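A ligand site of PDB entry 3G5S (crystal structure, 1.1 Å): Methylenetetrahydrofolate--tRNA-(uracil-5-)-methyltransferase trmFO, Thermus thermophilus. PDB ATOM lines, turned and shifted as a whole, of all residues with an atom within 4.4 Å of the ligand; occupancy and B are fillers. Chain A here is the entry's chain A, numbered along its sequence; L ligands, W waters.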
ATOM      1  N   VAL A   7     -39.263  13.732 -26.533  1.00  0.00           N
ATOM      2  CA  VAL A   7     -38.554  13.134 -27.648  1.00  0.00           C
ATOM      3  C   VAL A   7     -37.081  13.024 -27.308  1.00  0.00           C
ATOM      4  O   VAL A   7     -36.364  14.033 -27.238  1.00  0.00           O
ATOM      5  CB  VAL A   7     -38.755  13.924 -28.961  1.00  0.00           C
ATOM      6  CG1 VAL A   7     -38.064  13.215 -30.111  1.00  0.00           C
ATOM      7  CG2 VAL A   7     -40.249  14.120 -29.248  1.00  0.00           C
ATOM      8  N   GLY A   8     -36.636  11.790 -27.093  1.00  0.00           N
ATOM      9  CA  GLY A   8     -35.259  11.506 -26.699  1.00  0.00           C
ATOM     10  C   GLY A   8     -35.205  11.130 -25.235  1.00  0.00           C
ATOM     11  O   GLY A   8     -35.645  11.905 -24.382  1.00  0.00           O
ATOM     12  N   ALA A   9     -34.673   9.944 -24.934  1.00  0.00           N
ATOM     13  CA  ALA A   9     -34.565   9.453 -23.561  1.00  0.00           C
ATOM     14  C   ALA A   9     -33.112   9.438 -23.098  1.00  0.00           C
ATOM     15  O   ALA A   9     -32.626   8.440 -22.558  1.00  0.00           O
ATOM     16  CB  ALA A   9     -35.183   8.077 -23.440  1.00  0.00           C
ATOM     17  N   GLY A  10     -32.415  10.547 -23.320  1.00  0.00           N
ATOM     18  CA  GLY A  10     -31.073  10.724 -22.804  1.00  0.00           C
ATOM     19  C   GLY A  10     -31.104  11.396 -21.440  1.00  0.00           C
ATOM     20  O   GLY A  10     -32.039  11.212 -20.652  1.00  0.00           O
ATOM     21  N   LEU A  11     -30.082  12.173 -21.140  1.00  0.00           N
ATOM     22  CA  LEU A  11     -30.003  12.854 -19.849  1.00  0.00           C
ATOM     23  C   LEU A  11     -31.173  13.829 -19.660  1.00  0.00           C
ATOM     24  O   LEU A  11     -31.864  13.814 -18.633  1.00  0.00           O
ATOM     25  CB  LEU A  11     -28.668  13.584 -19.709  1.00  0.00           C
ATOM     26  CG  LEU A  11     -27.469  12.768 -19.228  1.00  0.00           C
ATOM     27  CD1 LEU A  11     -27.580  12.437 -17.740  1.00  0.00           C
ATOM     28  CD2 LEU A  11     -27.251  11.496 -20.047  1.00  0.00           C
ATOM     29  N   ALA A  12     -31.397  14.688 -20.661  1.00  0.00           N
ATOM     30  CA  ALA A  12     -32.439  15.692 -20.570  1.00  0.00           C
ATOM     31  C   ALA A  12     -33.838  15.098 -20.614  1.00  0.00           C
ATOM     32  O   ALA A  12     -34.704  15.470 -19.824  1.00  0.00           O
ATOM     33  CB  ALA A  12     -32.269  16.744 -21.658  1.00  0.00           C
ATOM     34  N   GLY A  13     -34.074  14.190 -21.552  1.00  0.00           N
ATOM     35  CA  GLY A  13     -35.408  13.649 -21.739  1.00  0.00           C
ATOM     36  C   GLY A  13     -35.824  12.791 -20.562  1.00  0.00           C
ATOM     37  O   GLY A  13     -36.996  12.787 -20.175  1.00  0.00           O
ATOM     38  N   PHE A  30     -40.318   8.988 -26.411  1.00  0.00           N
ATOM     39  CA  PHE A  30     -39.811   8.409 -27.648  1.00  0.00           C
ATOM     40  C   PHE A  30     -38.309   8.218 -27.562  1.00  0.00           C
ATOM     41  O   PHE A  30     -37.580   9.131 -27.164  1.00  0.00           O
ATOM     42  CB  PHE A  30     -40.094   9.324 -28.842  1.00  0.00           C
ATOM     43  CG  PHE A  30     -41.557   9.497 -29.184  1.00  0.00           C
ATOM     44  CD1 PHE A  30     -42.308  10.490 -28.579  1.00  0.00           C
ATOM     45  CD2 PHE A  30     -42.151   8.697 -30.140  1.00  0.00           C
ATOM     46  CE1 PHE A  30     -43.633  10.660 -28.900  1.00  0.00           C
ATOM     47  CE2 PHE A  30     -43.483   8.865 -30.468  1.00  0.00           C
ATOM     48  CZ  PHE A  30     -44.225   9.850 -29.855  1.00  0.00           C
ATOM     49  N   GLU A  31     -37.844   7.048 -27.961  1.00  0.00           N
ATOM     50  CA  GLU A  31     -36.421   6.781 -28.035  1.00  0.00           C
ATOM     51  C   GLU A  31     -36.158   5.850 -29.201  1.00  0.00           C
ATOM     52  O   GLU A  31     -36.732   4.761 -29.290  1.00  0.00           O
ATOM     53  CB  GLU A  31     -35.912   6.158 -26.726  1.00  0.00           C
ATOM     54  CG  GLU A  31     -34.443   5.760 -26.760  1.00  0.00           C
ATOM     55  CD  GLU A  31     -33.548   6.880 -27.248  1.00  0.00           C
ATOM     56  OE1 GLU A  31     -32.857   6.690 -28.270  1.00  0.00           O
ATOM     57  OE2 GLU A  31     -33.538   7.965 -26.591  1.00  0.00           O
ATOM     58  N   MET A  32     -35.275   6.265 -30.099  1.00  0.00           N
ATOM     59  CA  MET A  32     -35.003   5.446 -31.281  1.00  0.00           C
ATOM     60  C   MET A  32     -34.044   4.281 -31.014  1.00  0.00           C
ATOM     61  O   MET A  32     -34.039   3.300 -31.751  1.00  0.00           O
ATOM     62  CB  MET A  32     -34.489   6.327 -32.419  1.00  0.00           C
ATOM     63  CG  MET A  32     -33.119   6.912 -32.181  1.00  0.00           C
ATOM     64  SD  MET A  32     -32.655   8.112 -33.619  1.00  0.00           S
ATOM     65  CE  MET A  32     -30.813   8.473 -33.089  1.00  0.00           C
ATOM     66  N   ARG A  33     -33.220   4.396 -29.972  1.00  0.00           N
ATOM     67  CA  ARG A  33     -32.349   3.300 -29.607  1.00  0.00           C
ATOM     68  C   ARG A  33     -33.188   2.161 -29.038  1.00  0.00           C
ATOM     69  O   ARG A  33     -34.223   2.398 -28.414  1.00  0.00           O
ATOM     70  CB  ARG A  33     -31.327   3.757 -28.571  1.00  0.00           C
ATOM     71  CG  ARG A  33     -30.355   4.802 -29.099  1.00  0.00           C
ATOM     72  CD  ARG A  33     -29.345   5.209 -28.035  1.00  0.00           C
ATOM     73  NE  ARG A  33     -29.899   6.025 -26.958  1.00  0.00           N
ATOM     74  CZ  ARG A  33     -30.083   5.618 -25.709  1.00  0.00           C
ATOM     75  NH1 ARG A  33     -29.798   4.375 -25.355  1.00  0.00           N
ATOM     76  NH2 ARG A  33     -30.568   6.454 -24.799  1.00  0.00           N
ATOM     77  N   THR A  38     -27.163   6.300 -32.318  1.00  0.00           N
ATOM     78  CA  THR A  38     -26.337   7.422 -32.692  1.00  0.00           C
ATOM     79  C   THR A  38     -24.917   6.882 -32.807  1.00  0.00           C
ATOM     80  O   THR A  38     -24.632   5.783 -32.366  1.00  0.00           O
ATOM     81  CB  THR A  38     -26.325   8.496 -31.591  1.00  0.00           C
ATOM     82  OG1 THR A  38     -25.482   8.054 -30.523  1.00  0.00           O
ATOM     83  CG2 THR A  38     -27.733   8.757 -31.059  1.00  0.00           C
ATOM     84  N   ALA A  40     -22.498   7.578 -31.021  1.00  0.00           N
ATOM     85  CA  ALA A  40     -21.848   7.545 -29.708  1.00  0.00           C
ATOM     86  C   ALA A  40     -22.447   6.546 -28.725  1.00  0.00           C
ATOM     87  O   ALA A  40     -21.806   6.180 -27.737  1.00  0.00           O
ATOM     88  CB  ALA A  40     -21.815   8.945 -29.101  1.00  0.00           C
ATOM     89  N   HIS A  41     -23.678   6.107 -28.977  1.00  0.00           N
ATOM     90  CA  HIS A  41     -24.394   5.234 -28.046  1.00  0.00           C
ATOM     91  C   HIS A  41     -24.189   3.762 -28.359  1.00  0.00           C
ATOM     92  O   HIS A  41     -23.919   3.408 -29.512  1.00  0.00           O
ATOM     93  CB  HIS A  41     -25.890   5.521 -28.110  1.00  0.00           C
ATOM     94  CG  HIS A  41     -26.307   6.764 -27.385  1.00  0.00           C
ATOM     95  ND1 HIS A  41     -26.206   8.019 -27.936  1.00  0.00           N
ATOM     96  CD2 HIS A  41     -26.836   6.929 -26.155  1.00  0.00           C
ATOM     97  CE1 HIS A  41     -26.658   8.906 -27.076  1.00  0.00           C
ATOM     98  NE2 HIS A  41     -27.045   8.277 -25.988  1.00  0.00           N
ATOM     99  N   VAL A  50     -22.348   8.444 -22.498  1.00  0.00           N
ATOM    100  CA  VAL A  50     -21.589   8.001 -23.670  1.00  0.00           C
ATOM    101  C   VAL A  50     -20.070   8.164 -23.568  1.00  0.00           C
ATOM    102  O   VAL A  50     -19.331   7.575 -24.349  1.00  0.00           O
ATOM    103  CB  VAL A  50     -22.092   8.634 -24.988  1.00  0.00           C
ATOM    104  CG1 VAL A  50     -23.551   8.269 -25.220  1.00  0.00           C
ATOM    105  CG2 VAL A  50     -21.880  10.128 -24.980  1.00  0.00           C
ATOM    106  N   CYS A  51     -19.589   8.954 -22.609  1.00  0.00           N
ATOM    107  CA  CYS A  51     -18.151   9.205 -22.511  1.00  0.00           C
ATOM    108  C   CYS A  51     -17.665   9.150 -21.065  1.00  0.00           C
ATOM    109  O   CYS A  51     -17.826   8.135 -20.397  1.00  0.00           O
ATOM    110  CB  CYS A  51     -17.801  10.543 -23.154  1.00  0.00           C
ATOM    111  SG  CYS A  51     -16.067  10.729 -23.620  1.00  0.00           S
ATOM    112  N   SER A  52     -17.071  10.234 -20.583  1.00  0.00           N
ATOM    113  CA  SER A  52     -16.577  10.283 -19.209  1.00  0.00           C
ATOM    114  C   SER A  52     -17.702   9.989 -18.232  1.00  0.00           C
ATOM    115  O   SER A  52     -18.853  10.322 -18.491  1.00  0.00           O
ATOM    116  CB  SER A  52     -15.957  11.638 -18.885  1.00  0.00           C
ATOM    117  OG  SER A  52     -15.698  11.760 -17.497  1.00  0.00           O
ATOM    118  N   GLU A 119     -39.133   4.449 -31.364  1.00  0.00           N
ATOM    119  CA  GLU A 119     -39.187   4.878 -32.743  1.00  0.00           C
ATOM    120  C   GLU A 119     -38.428   6.181 -32.899  1.00  0.00           C
ATOM    121  O   GLU A 119     -38.211   6.915 -31.930  1.00  0.00           O
ATOM    122  CB  GLU A 119     -40.631   5.050 -33.192  1.00  0.00           C
ATOM    123  CG  GLU A 119     -41.269   6.379 -32.827  1.00  0.00           C
ATOM    124  CD  GLU A 119     -42.590   6.619 -33.542  1.00  0.00           C
ATOM    125  OE1 GLU A 119     -42.840   7.768 -33.962  1.00  0.00           O
ATOM    126  OE2 GLU A 119     -43.366   5.652 -33.683  1.00  0.00           O
ATOM    127  N   GLU A 120     -37.997   6.451 -34.124  1.00  0.00           N
ATOM    128  CA  GLU A 120     -37.405   7.732 -34.453  1.00  0.00           C
ATOM    129  C   GLU A 120     -38.521   8.719 -34.766  1.00  0.00           C
ATOM    130  O   GLU A 120     -39.370   8.452 -35.616  1.00  0.00           O
ATOM    131  CB  GLU A 120     -36.491   7.628 -35.673  1.00  0.00           C
ATOM    132  CG  GLU A 120     -35.882   8.970 -36.026  1.00  0.00           C
ATOM    133  CD  GLU A 120     -35.353   9.057 -37.440  1.00  0.00           C
ATOM    134  OE1 GLU A 120     -35.575   8.128 -38.254  1.00  0.00           O
ATOM    135  OE2 GLU A 120     -34.733  10.100 -37.752  1.00  0.00           O
ATOM    136  N   VAL A 121     -38.499   9.860 -34.095  1.00  0.00           N
ATOM    137  CA  VAL A 121     -39.435  10.934 -34.385  1.00  0.00           C
ATOM    138  C   VAL A 121     -38.855  11.766 -35.517  1.00  0.00           C
ATOM    139  O   VAL A 121     -37.742  12.276 -35.416  1.00  0.00           O
ATOM    140  CB  VAL A 121     -39.684  11.799 -33.124  1.00  0.00           C
ATOM    141  CG1 VAL A 121     -40.499  13.032 -33.459  1.00  0.00           C
ATOM    142  CG2 VAL A 121     -40.364  10.950 -32.061  1.00  0.00           C
ATOM    143  N   ALA A 132     -35.644  16.717 -26.840  1.00  0.00           N
ATOM    144  CA  ALA A 132     -34.433  16.467 -26.051  1.00  0.00           C
ATOM    145  C   ALA A 132     -33.537  15.446 -26.752  1.00  0.00           C
ATOM    146  O   ALA A 132     -33.120  14.441 -26.168  1.00  0.00           O
ATOM    147  CB  ALA A 132     -34.810  15.996 -24.642  1.00  0.00           C
ATOM    148  N   THR A 133     -33.234  15.707 -28.018  1.00  0.00           N
ATOM    149  CA  THR A 133     -32.626  14.704 -28.884  1.00  0.00           C
ATOM    150  C   THR A 133     -31.100  14.754 -28.945  1.00  0.00           C
ATOM    151  O   THR A 133     -30.484  13.906 -29.590  1.00  0.00           O
ATOM    152  CB  THR A 133     -33.261  14.760 -30.279  1.00  0.00           C
ATOM    153  OG1 THR A 133     -33.391  16.127 -30.687  1.00  0.00           O
ATOM    154  CG2 THR A 133     -34.652  14.138 -30.234  1.00  0.00           C
ATOM    155  N   GLY A 134     -30.487  15.725 -28.269  1.00  0.00           N
ATOM    156  CA  GLY A 134     -29.070  15.678 -27.994  1.00  0.00           C
ATOM    157  C   GLY A 134     -28.147  16.111 -29.116  1.00  0.00           C
ATOM    158  O   GLY A 134     -28.574  16.557 -30.174  1.00  0.00           O
ATOM    159  N   PRO A 135     -26.843  15.968 -28.871  1.00  0.00           N
ATOM    160  CA  PRO A 135     -25.842  16.392 -29.864  1.00  0.00           C
ATOM    161  C   PRO A 135     -25.927  15.616 -31.163  1.00  0.00           C
ATOM    162  O   PRO A 135     -25.488  16.129 -32.193  1.00  0.00           O
ATOM    163  CB  PRO A 135     -24.519  16.099 -29.162  1.00  0.00           C
ATOM    164  CG  PRO A 135     -24.824  15.064 -28.148  1.00  0.00           C
ATOM    165  CD  PRO A 135     -26.227  15.326 -27.695  1.00  0.00           C
ATOM    166  N   LEU A 136     -26.484  14.414 -31.130  1.00  0.00           N
ATOM    167  CA  LEU A 136     -26.597  13.578 -32.306  1.00  0.00           C
ATOM    168  C   LEU A 136     -28.079  13.366 -32.666  1.00  0.00           C
ATOM    169  O   LEU A 136     -28.509  12.299 -33.088  1.00  0.00           O
ATOM    170  CB  LEU A 136     -25.863  12.252 -32.094  1.00  0.00           C
ATOM    171  CG  LEU A 136     -24.377  12.438 -31.774  1.00  0.00           C
ATOM    172  CD1 LEU A 136     -23.711  11.131 -31.335  1.00  0.00           C
ATOM    173  CD2 LEU A 136     -23.639  13.056 -32.956  1.00  0.00           C
ATOM    174  N   THR A 137     -28.844  14.442 -32.487  1.00  0.00           N
ATOM    175  CA  THR A 137     -30.219  14.540 -32.969  1.00  0.00           C
ATOM    176  C   THR A 137     -30.302  13.946 -34.371  1.00  0.00           C
ATOM    177  O   THR A 137     -29.476  14.243 -35.232  1.00  0.00           O
ATOM    178  CB  THR A 137     -30.671  16.013 -33.003  1.00  0.00           C
ATOM    179  OG1 THR A 137     -30.860  16.508 -31.671  1.00  0.00           O
ATOM    180  CG2 THR A 137     -31.958  16.172 -33.758  1.00  0.00           C
ATOM    181  N   SER A 138     -31.305  13.106 -34.627  1.00  0.00           N
ATOM    182  CA  SER A 138     -31.396  12.452 -35.929  1.00  0.00           C
ATOM    183  C   SER A 138     -31.540  13.485 -37.040  1.00  0.00           C
ATOM    184  O   SER A 138     -32.111  14.565 -36.855  1.00  0.00           O
ATOM    185  CB  SER A 138     -32.551  11.449 -35.976  1.00  0.00           C
ATOM    186  OG  SER A 138     -33.773  12.111 -36.207  1.00  0.00           O
ATOM    187  N   LEU A 141     -35.131  14.829 -37.798  1.00  0.00           N
ATOM    188  CA  LEU A 141     -35.692  15.816 -36.887  1.00  0.00           C
ATOM    189  C   LEU A 141     -34.975  17.157 -37.011  1.00  0.00           C
ATOM    190  O   LEU A 141     -35.603  18.215 -36.923  1.00  0.00           O
ATOM    191  CB  LEU A 141     -35.683  15.327 -35.442  1.00  0.00           C
ATOM    192  CG  LEU A 141     -36.444  16.234 -34.476  1.00  0.00           C
ATOM    193  CD1 LEU A 141     -37.922  16.293 -34.809  1.00  0.00           C
ATOM    194  CD2 LEU A 141     -36.228  15.748 -33.055  1.00  0.00           C
ATOM    195  N   HIS A 212     -13.351  12.463 -32.478  1.00  0.00           N
ATOM    196  CA  HIS A 212     -13.943  11.128 -32.469  1.00  0.00           C
ATOM    197  C   HIS A 212     -14.009  10.595 -33.894  1.00  0.00           C
ATOM    198  O   HIS A 212     -14.017  11.375 -34.858  1.00  0.00           O
ATOM    199  CB  HIS A 212     -15.343  11.155 -31.856  1.00  0.00           C
ATOM    200  CG  HIS A 212     -15.392  11.724 -30.470  1.00  0.00           C
ATOM    201  ND1 HIS A 212     -15.029  10.997 -29.360  1.00  0.00           N
ATOM    202  CD2 HIS A 212     -15.758  12.948 -30.029  1.00  0.00           C
ATOM    203  CE1 HIS A 212     -15.171  11.754 -28.278  1.00  0.00           C
ATOM    204  NE2 HIS A 212     -15.612  12.935 -28.658  1.00  0.00           N
ATOM    205  N   GLY A 335     -31.550  20.006 -22.888  1.00  0.00           N
ATOM    206  CA  GLY A 335     -30.304  19.321 -23.160  1.00  0.00           C
ATOM    207  C   GLY A 335     -29.486  20.043 -24.207  1.00  0.00           C
ATOM    208  O   GLY A 335     -29.639  21.245 -24.435  1.00  0.00           O
ATOM    209  N   VAL A 336     -28.573  19.312 -24.827  1.00  0.00           N
ATOM    210  CA  VAL A 336     -27.692  19.887 -25.833  1.00  0.00           C
ATOM    211  C   VAL A 336     -28.487  20.576 -26.957  1.00  0.00           C
ATOM    212  O   VAL A 336     -28.073  21.606 -27.465  1.00  0.00           O
ATOM    213  CB  VAL A 336     -26.734  18.826 -26.380  1.00  0.00           C
ATOM    214  CG1 VAL A 336     -26.071  19.281 -27.682  1.00  0.00           C
ATOM    215  CG2 VAL A 336     -25.696  18.499 -25.329  1.00  0.00           C
ATOM    216  N   GLU A 341     -24.282  22.288 -22.539  1.00  0.00           N
ATOM    217  CA  GLU A 341     -23.280  21.262 -22.656  1.00  0.00           C
ATOM    218  C   GLU A 341     -23.090  20.664 -21.276  1.00  0.00           C
ATOM    219  O   GLU A 341     -22.987  21.400 -20.293  1.00  0.00           O
ATOM    220  CB  GLU A 341     -21.964  21.864 -23.133  1.00  0.00           C
ATOM    221  CG  GLU A 341     -20.729  20.995 -22.937  1.00  0.00           C
ATOM    222  CD  GLU A 341     -20.794  19.674 -23.670  1.00  0.00           C
ATOM    223  OE1 GLU A 341     -21.698  19.479 -24.514  1.00  0.00           O
ATOM    224  OE2 GLU A 341     -19.918  18.822 -23.402  1.00  0.00           O
ATOM    225  N   GLY A 342     -23.041  19.329 -21.208  1.00  0.00           N
ATOM    226  CA  GLY A 342     -22.750  18.626 -19.972  1.00  0.00           C
ATOM    227  C   GLY A 342     -23.908  17.728 -19.548  1.00  0.00           C
ATOM    228  O   GLY A 342     -25.081  18.078 -19.730  1.00  0.00           O
ATOM    229  N   TYR A 343     -23.582  16.586 -18.958  1.00  0.00           N
ATOM    230  CA  TYR A 343     -24.634  15.656 -18.530  1.00  0.00           C
ATOM    231  C   TYR A 343     -25.597  16.322 -17.558  1.00  0.00           C
ATOM    232  O   TYR A 343     -26.816  16.209 -17.691  1.00  0.00           O
ATOM    233  CB  TYR A 343     -24.078  14.401 -17.863  1.00  0.00           C
ATOM    234  CG  TYR A 343     -23.045  13.608 -18.647  1.00  0.00           C
ATOM    235  CD1 TYR A 343     -23.327  13.071 -19.891  1.00  0.00           C
ATOM    236  CD2 TYR A 343     -21.800  13.364 -18.087  1.00  0.00           C
ATOM    237  CE1 TYR A 343     -22.371  12.329 -20.582  1.00  0.00           C
ATOM    238  CE2 TYR A 343     -20.851  12.623 -18.756  1.00  0.00           C
ATOM    239  CZ  TYR A 343     -21.136  12.106 -20.003  1.00  0.00           C
ATOM    240  OH  TYR A 343     -20.180  11.367 -20.666  1.00  0.00           O
ATOM    241  N   SER A 346     -27.664  19.142 -18.979  1.00  0.00           N
ATOM    242  CA  SER A 346     -28.716  18.565 -19.799  1.00  0.00           C
ATOM    243  C   SER A 346     -29.866  18.068 -18.923  1.00  0.00           C
ATOM    244  O   SER A 346     -31.022  18.389 -19.187  1.00  0.00           O
ATOM    245  CB  SER A 346     -28.129  17.473 -20.688  1.00  0.00           C
ATOM    246  OG  SER A 346     -27.222  18.031 -21.628  1.00  0.00           O
HETATM  247  P1  LIG L   1     -28.449  12.538 -25.213  1.00  0.00           P
HETATM  248  O1  LIG L   1     -27.554  12.223 -26.375  1.00  0.00           O
HETATM  249  O2  LIG L   1     -28.054  12.045 -23.856  1.00  0.00           O
HETATM  250  O3  LIG L   1     -29.941  12.029 -25.482  1.00  0.00           O
HETATM  251  C1  LIG L   1     -30.578  12.249 -26.721  1.00  0.00           C
HETATM  252  C2  LIG L   1     -31.453  11.039 -27.006  1.00  0.00           C
HETATM  253  O4  LIG L   1     -32.274  11.303 -28.128  1.00  0.00           O
HETATM  254  C3  LIG L   1     -30.611   9.819 -27.366  1.00  0.00           C
HETATM  255  O5  LIG L   1     -30.980   8.703 -26.568  1.00  0.00           O
HETATM  256  C4  LIG L   1     -30.916   9.574 -28.843  1.00  0.00           C
HETATM  257  O6  LIG L   1     -30.886   8.224 -29.236  1.00  0.00           O
HETATM  258  C5  LIG L   1     -32.313  10.147 -28.968  1.00  0.00           C
HETATM  259  N1  LIG L   1     -32.735  10.641 -30.282  1.00  0.00           N
HETATM  260  C6  LIG L   1     -32.052  11.468 -31.136  1.00  0.00           C
HETATM  261  N2  LIG L   1     -32.846  11.757 -32.190  1.00  0.00           N
HETATM  262  C7  LIG L   1     -34.030  11.129 -32.003  1.00  0.00           C
HETATM  263  C8  LIG L   1     -35.207  11.074 -32.743  1.00  0.00           C
HETATM  264  N3  LIG L   1     -35.420  11.853 -33.819  1.00  0.00           N
HETATM  265  N4  LIG L   1     -36.247  10.329 -32.255  1.00  0.00           N
HETATM  266  C9  LIG L   1     -36.146   9.636 -31.076  1.00  0.00           C
HETATM  267  N5  LIG L   1     -34.990   9.688 -30.328  1.00  0.00           N
HETATM  268  C10 LIG L   1     -33.971  10.431 -30.808  1.00  0.00           C
HETATM  269  N6  LIG L   1     -20.889  15.553 -21.513  1.00  0.00           N
HETATM  270  C11 LIG L   1     -20.222  15.609 -20.319  1.00  0.00           C
HETATM  271  O7  LIG L   1     -20.671  16.250 -19.383  1.00  0.00           O
HETATM  272  N7  LIG L   1     -19.027  14.919 -20.183  1.00  0.00           N
HETATM  273  C12 LIG L   1     -18.476  14.172 -21.205  1.00  0.00           C
HETATM  274  O8  LIG L   1     -17.409  13.566 -21.037  1.00  0.00           O
HETATM  275  C13 LIG L   1     -19.172  14.119 -22.413  1.00  0.00           C
HETATM  276  N8  LIG L   1     -18.677  13.397 -23.474  1.00  0.00           N
HETATM  277  C14 LIG L   1     -19.375  13.356 -24.670  1.00  0.00           C
HETATM  278  C15 LIG L   1     -18.869  12.617 -25.721  1.00  0.00           C
HETATM  279  C16 LIG L   1     -19.543  12.557 -26.936  1.00  0.00           C
HETATM  280  C17 LIG L   1     -18.992  11.753 -28.072  1.00  0.00           C
HETATM  281  C18 LIG L   1     -20.752  13.244 -27.071  1.00  0.00           C
HETATM  282  C19 LIG L   1     -21.494  13.190 -28.379  1.00  0.00           C
HETATM  283  C20 LIG L   1     -21.266  13.993 -26.014  1.00  0.00           C
HETATM  284  C21 LIG L   1     -20.579  14.055 -24.800  1.00  0.00           C
HETATM  285  N9  LIG L   1     -21.079  14.806 -23.743  1.00  0.00           N
HETATM  286  C22 LIG L   1     -20.369  14.816 -22.565  1.00  0.00           C
HETATM  287  C23 LIG L   1     -21.932  16.016 -24.045  1.00  0.00           C
HETATM  288  C24 LIG L   1     -23.340  15.961 -23.428  1.00  0.00           C
HETATM  289  O9  LIG L   1     -23.347  16.409 -22.076  1.00  0.00           O
HETATM  290  C25 LIG L   1     -23.978  14.580 -23.548  1.00  0.00           C
HETATM  291  O10 LIG L   1     -24.143  14.331 -24.933  1.00  0.00           O
HETATM  292  C26 LIG L   1     -25.329  14.465 -22.837  1.00  0.00           C
HETATM  293  O11 LIG L   1     -25.693  13.099 -22.833  1.00  0.00           O
HETATM  294  C27 LIG L   1     -26.392  15.332 -23.505  1.00  0.00           C
HETATM  295  O12 LIG L   1     -27.666  14.989 -22.992  1.00  0.00           O
HETATM  296  P2  LIG L   1     -28.942  15.092 -23.946  1.00  0.00           P
HETATM  297  O13 LIG L   1     -29.071  16.467 -24.519  1.00  0.00           O
HETATM  298  O14 LIG L   1     -30.105  14.569 -23.167  1.00  0.00           O
HETATM  299  O15 LIG L   1     -28.598  14.134 -25.188  1.00  0.00           O
HETATM  300  O   HOH W   1     -16.235  15.326 -24.641  1.00  0.00           O
HETATM  301  O   HOH W   2     -18.376  16.937 -24.375  1.00  0.00           O
HETATM  302  O   HOH W   3     -22.096  17.735 -26.799  1.00  0.00           O
HETATM  303  O   HOH W   4     -17.675  14.680 -17.762  1.00  0.00           O
HETATM  304  O   HOH W   5     -30.959  17.564 -26.176  1.00  0.00           O
HETATM  305  O   HOH W   6     -24.867  11.757 -25.731  1.00  0.00           O
HETATM  306  O   HOH W   7     -32.475  13.402 -23.732  1.00  0.00           O
HETATM  307  O   HOH W   8     -27.867  12.722 -29.232  1.00  0.00           O
HETATM  308  O   HOH W   9     -24.494  10.598 -22.827  1.00  0.00           O
HETATM  309  O   HOH W  10     -18.890  18.444 -20.895  1.00  0.00           O
HETATM  310  O   HOH W  11     -28.040   9.275 -23.513  1.00  0.00           O
HETATM  311  O   HOH W  12     -19.988  16.239 -16.888  1.00  0.00           O
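The side-chain carboxylate (OE2) of Glu 31 sits at hydrogen-bond distance from an oxygen (O5) of the ligand, 2.7 Å away.
N of Ala 12 lies within hydrogen-bond range of O14 of the ligand (2.8 Å).
A nitrogen (N4) of the ligand lies within hydrogen-bond range of the backbone NH (N) of Val 121 (2.9 Å).
The backbone carbonyl oxygen of Val 121 is in hydrogen-bond range of a nitrogen (N3) of the ligand (2.8 Å).
O5 of the ligand sits at hydrogen-bond distance from NH2 of Arg 33.
An oxygen (O13) of the ligand lies within hydrogen-bond range of the backbone NH (N) of Val 336 (2.9 Å).
O9 of the ligand lies close to N of Gly 342 (3.1 Å).
An oxygen (O9) of the ligand sits close to the backbone carbonyl oxygen (O) of Gly 342.
N of Ser 138 lies within hydrogen-bond range of N2 of the ligand (3.2 Å).
OG of Ser 138 lies within hydrogen-bond range of N3 of the ligand (2.9 Å).
An oxygen (O7) of the ligand sits at hydrogen-bond distance from the backbone NH (N) of Tyr 343 (3.0 Å).
SG of Cys 51 sits close to N8 of the ligand, 3.7 Å away.
The backbone NH of Leu 11 sits at hydrogen-bond distance from an oxygen (O14) of the ligand (3.1 Å).
N of Ser 52 lies close to O8 of the ligand, 3.4 Å away.
The side-chain hydroxyl (OG) of Ser 346 is in hydrogen-bond range of an oxygen (O12) of the ligand (3.4 Å).
The backbone NH (N) of Met 32 lies within hydrogen-bond range of a nitrogen (N5) of the ligand, at 3.4 Å.
O of Glu 31 lies within hydrogen-bond range of N of Glu 119, at 3.2 Å.
The backbone carbonyl oxygen (O) of Gly 342 lies within hydrogen-bond range of the side-chain hydroxyl (OG) of Ser 346, at 2.9 Å.
OE2 of Glu 120 sits at hydrogen-bond distance from OG of Ser 138 (2.7 Å).
The backbone NH (N) of Cys 51 lies within hydrogen-bond range of the side-chain hydroxyl (OH) of Tyr 343 (3.2 Å).
The side-chain hydroxyl of Thr 137 is in hydrogen-bond range of the backbone carbonyl oxygen of Gly 134, at 2.7 Å.
OG1 of Thr 137 sits at hydrogen-bond distance from OG1 of Thr 133, at 2.7 Å.
N of Gly 8 sits at hydrogen-bond distance from O of Phe 30, 2.8 Å away.
A ring nitrogen (ND1) of His 41 lies within hydrogen-bond range of the side-chain hydroxyl of Thr 38 (2.7 Å).
An oxygen (O4) of the ligand sits close to the backbone carbonyl oxygen (O) of Thr 133 (3.5 Å).
Residues that only touch the ligand: Gly 10 (3.2 Å), Gly 134 (3.2 Å), Gly 8 (3.3 Å), Pro 135 (3.4 Å), Gly 335 (3.4 Å), Ala 132 (3.4 Å), Glu 341 (3.5 Å), His 41 (3.5 Å), Glu 119 (3.5 Å), Glu 120 (3.6 Å), His 212 (3.6 Å), Thr 38 (3.7 Å), Leu 141 (3.8 Å), Val 50 (3.9 Å), Thr 137 (3.9 Å) and Ala 9 (3.98 Å).
Of the 35 residues printed, 30 come within 4 Å of the ligand.
Along chain A the residues within 4 Å of the ligand span positions 8 to 346.
The nearest printed residue that does not touch the ligand is Val 7 (4.03 Å).
Water W9 lies within hydrogen-bond range of O11 of the ligand (2.8 Å) and N of Val 50 (3.1 Å).
Water W11 lies within hydrogen-bond range of O2 of the ligand (2.8 Å) and NE2 of His 41 (2.8 Å).
Water W8 lies within hydrogen-bond range of the backbone NH (N) of Leu 136, the backbone carbonyl oxygen (O) of Thr 133 and an oxygen (O1) of the ligand.
Water W10 bridges the side-chain carboxylate of Glu 341 (2.7 Å) and an oxygen (O7) of the ligand (3.2 Å).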
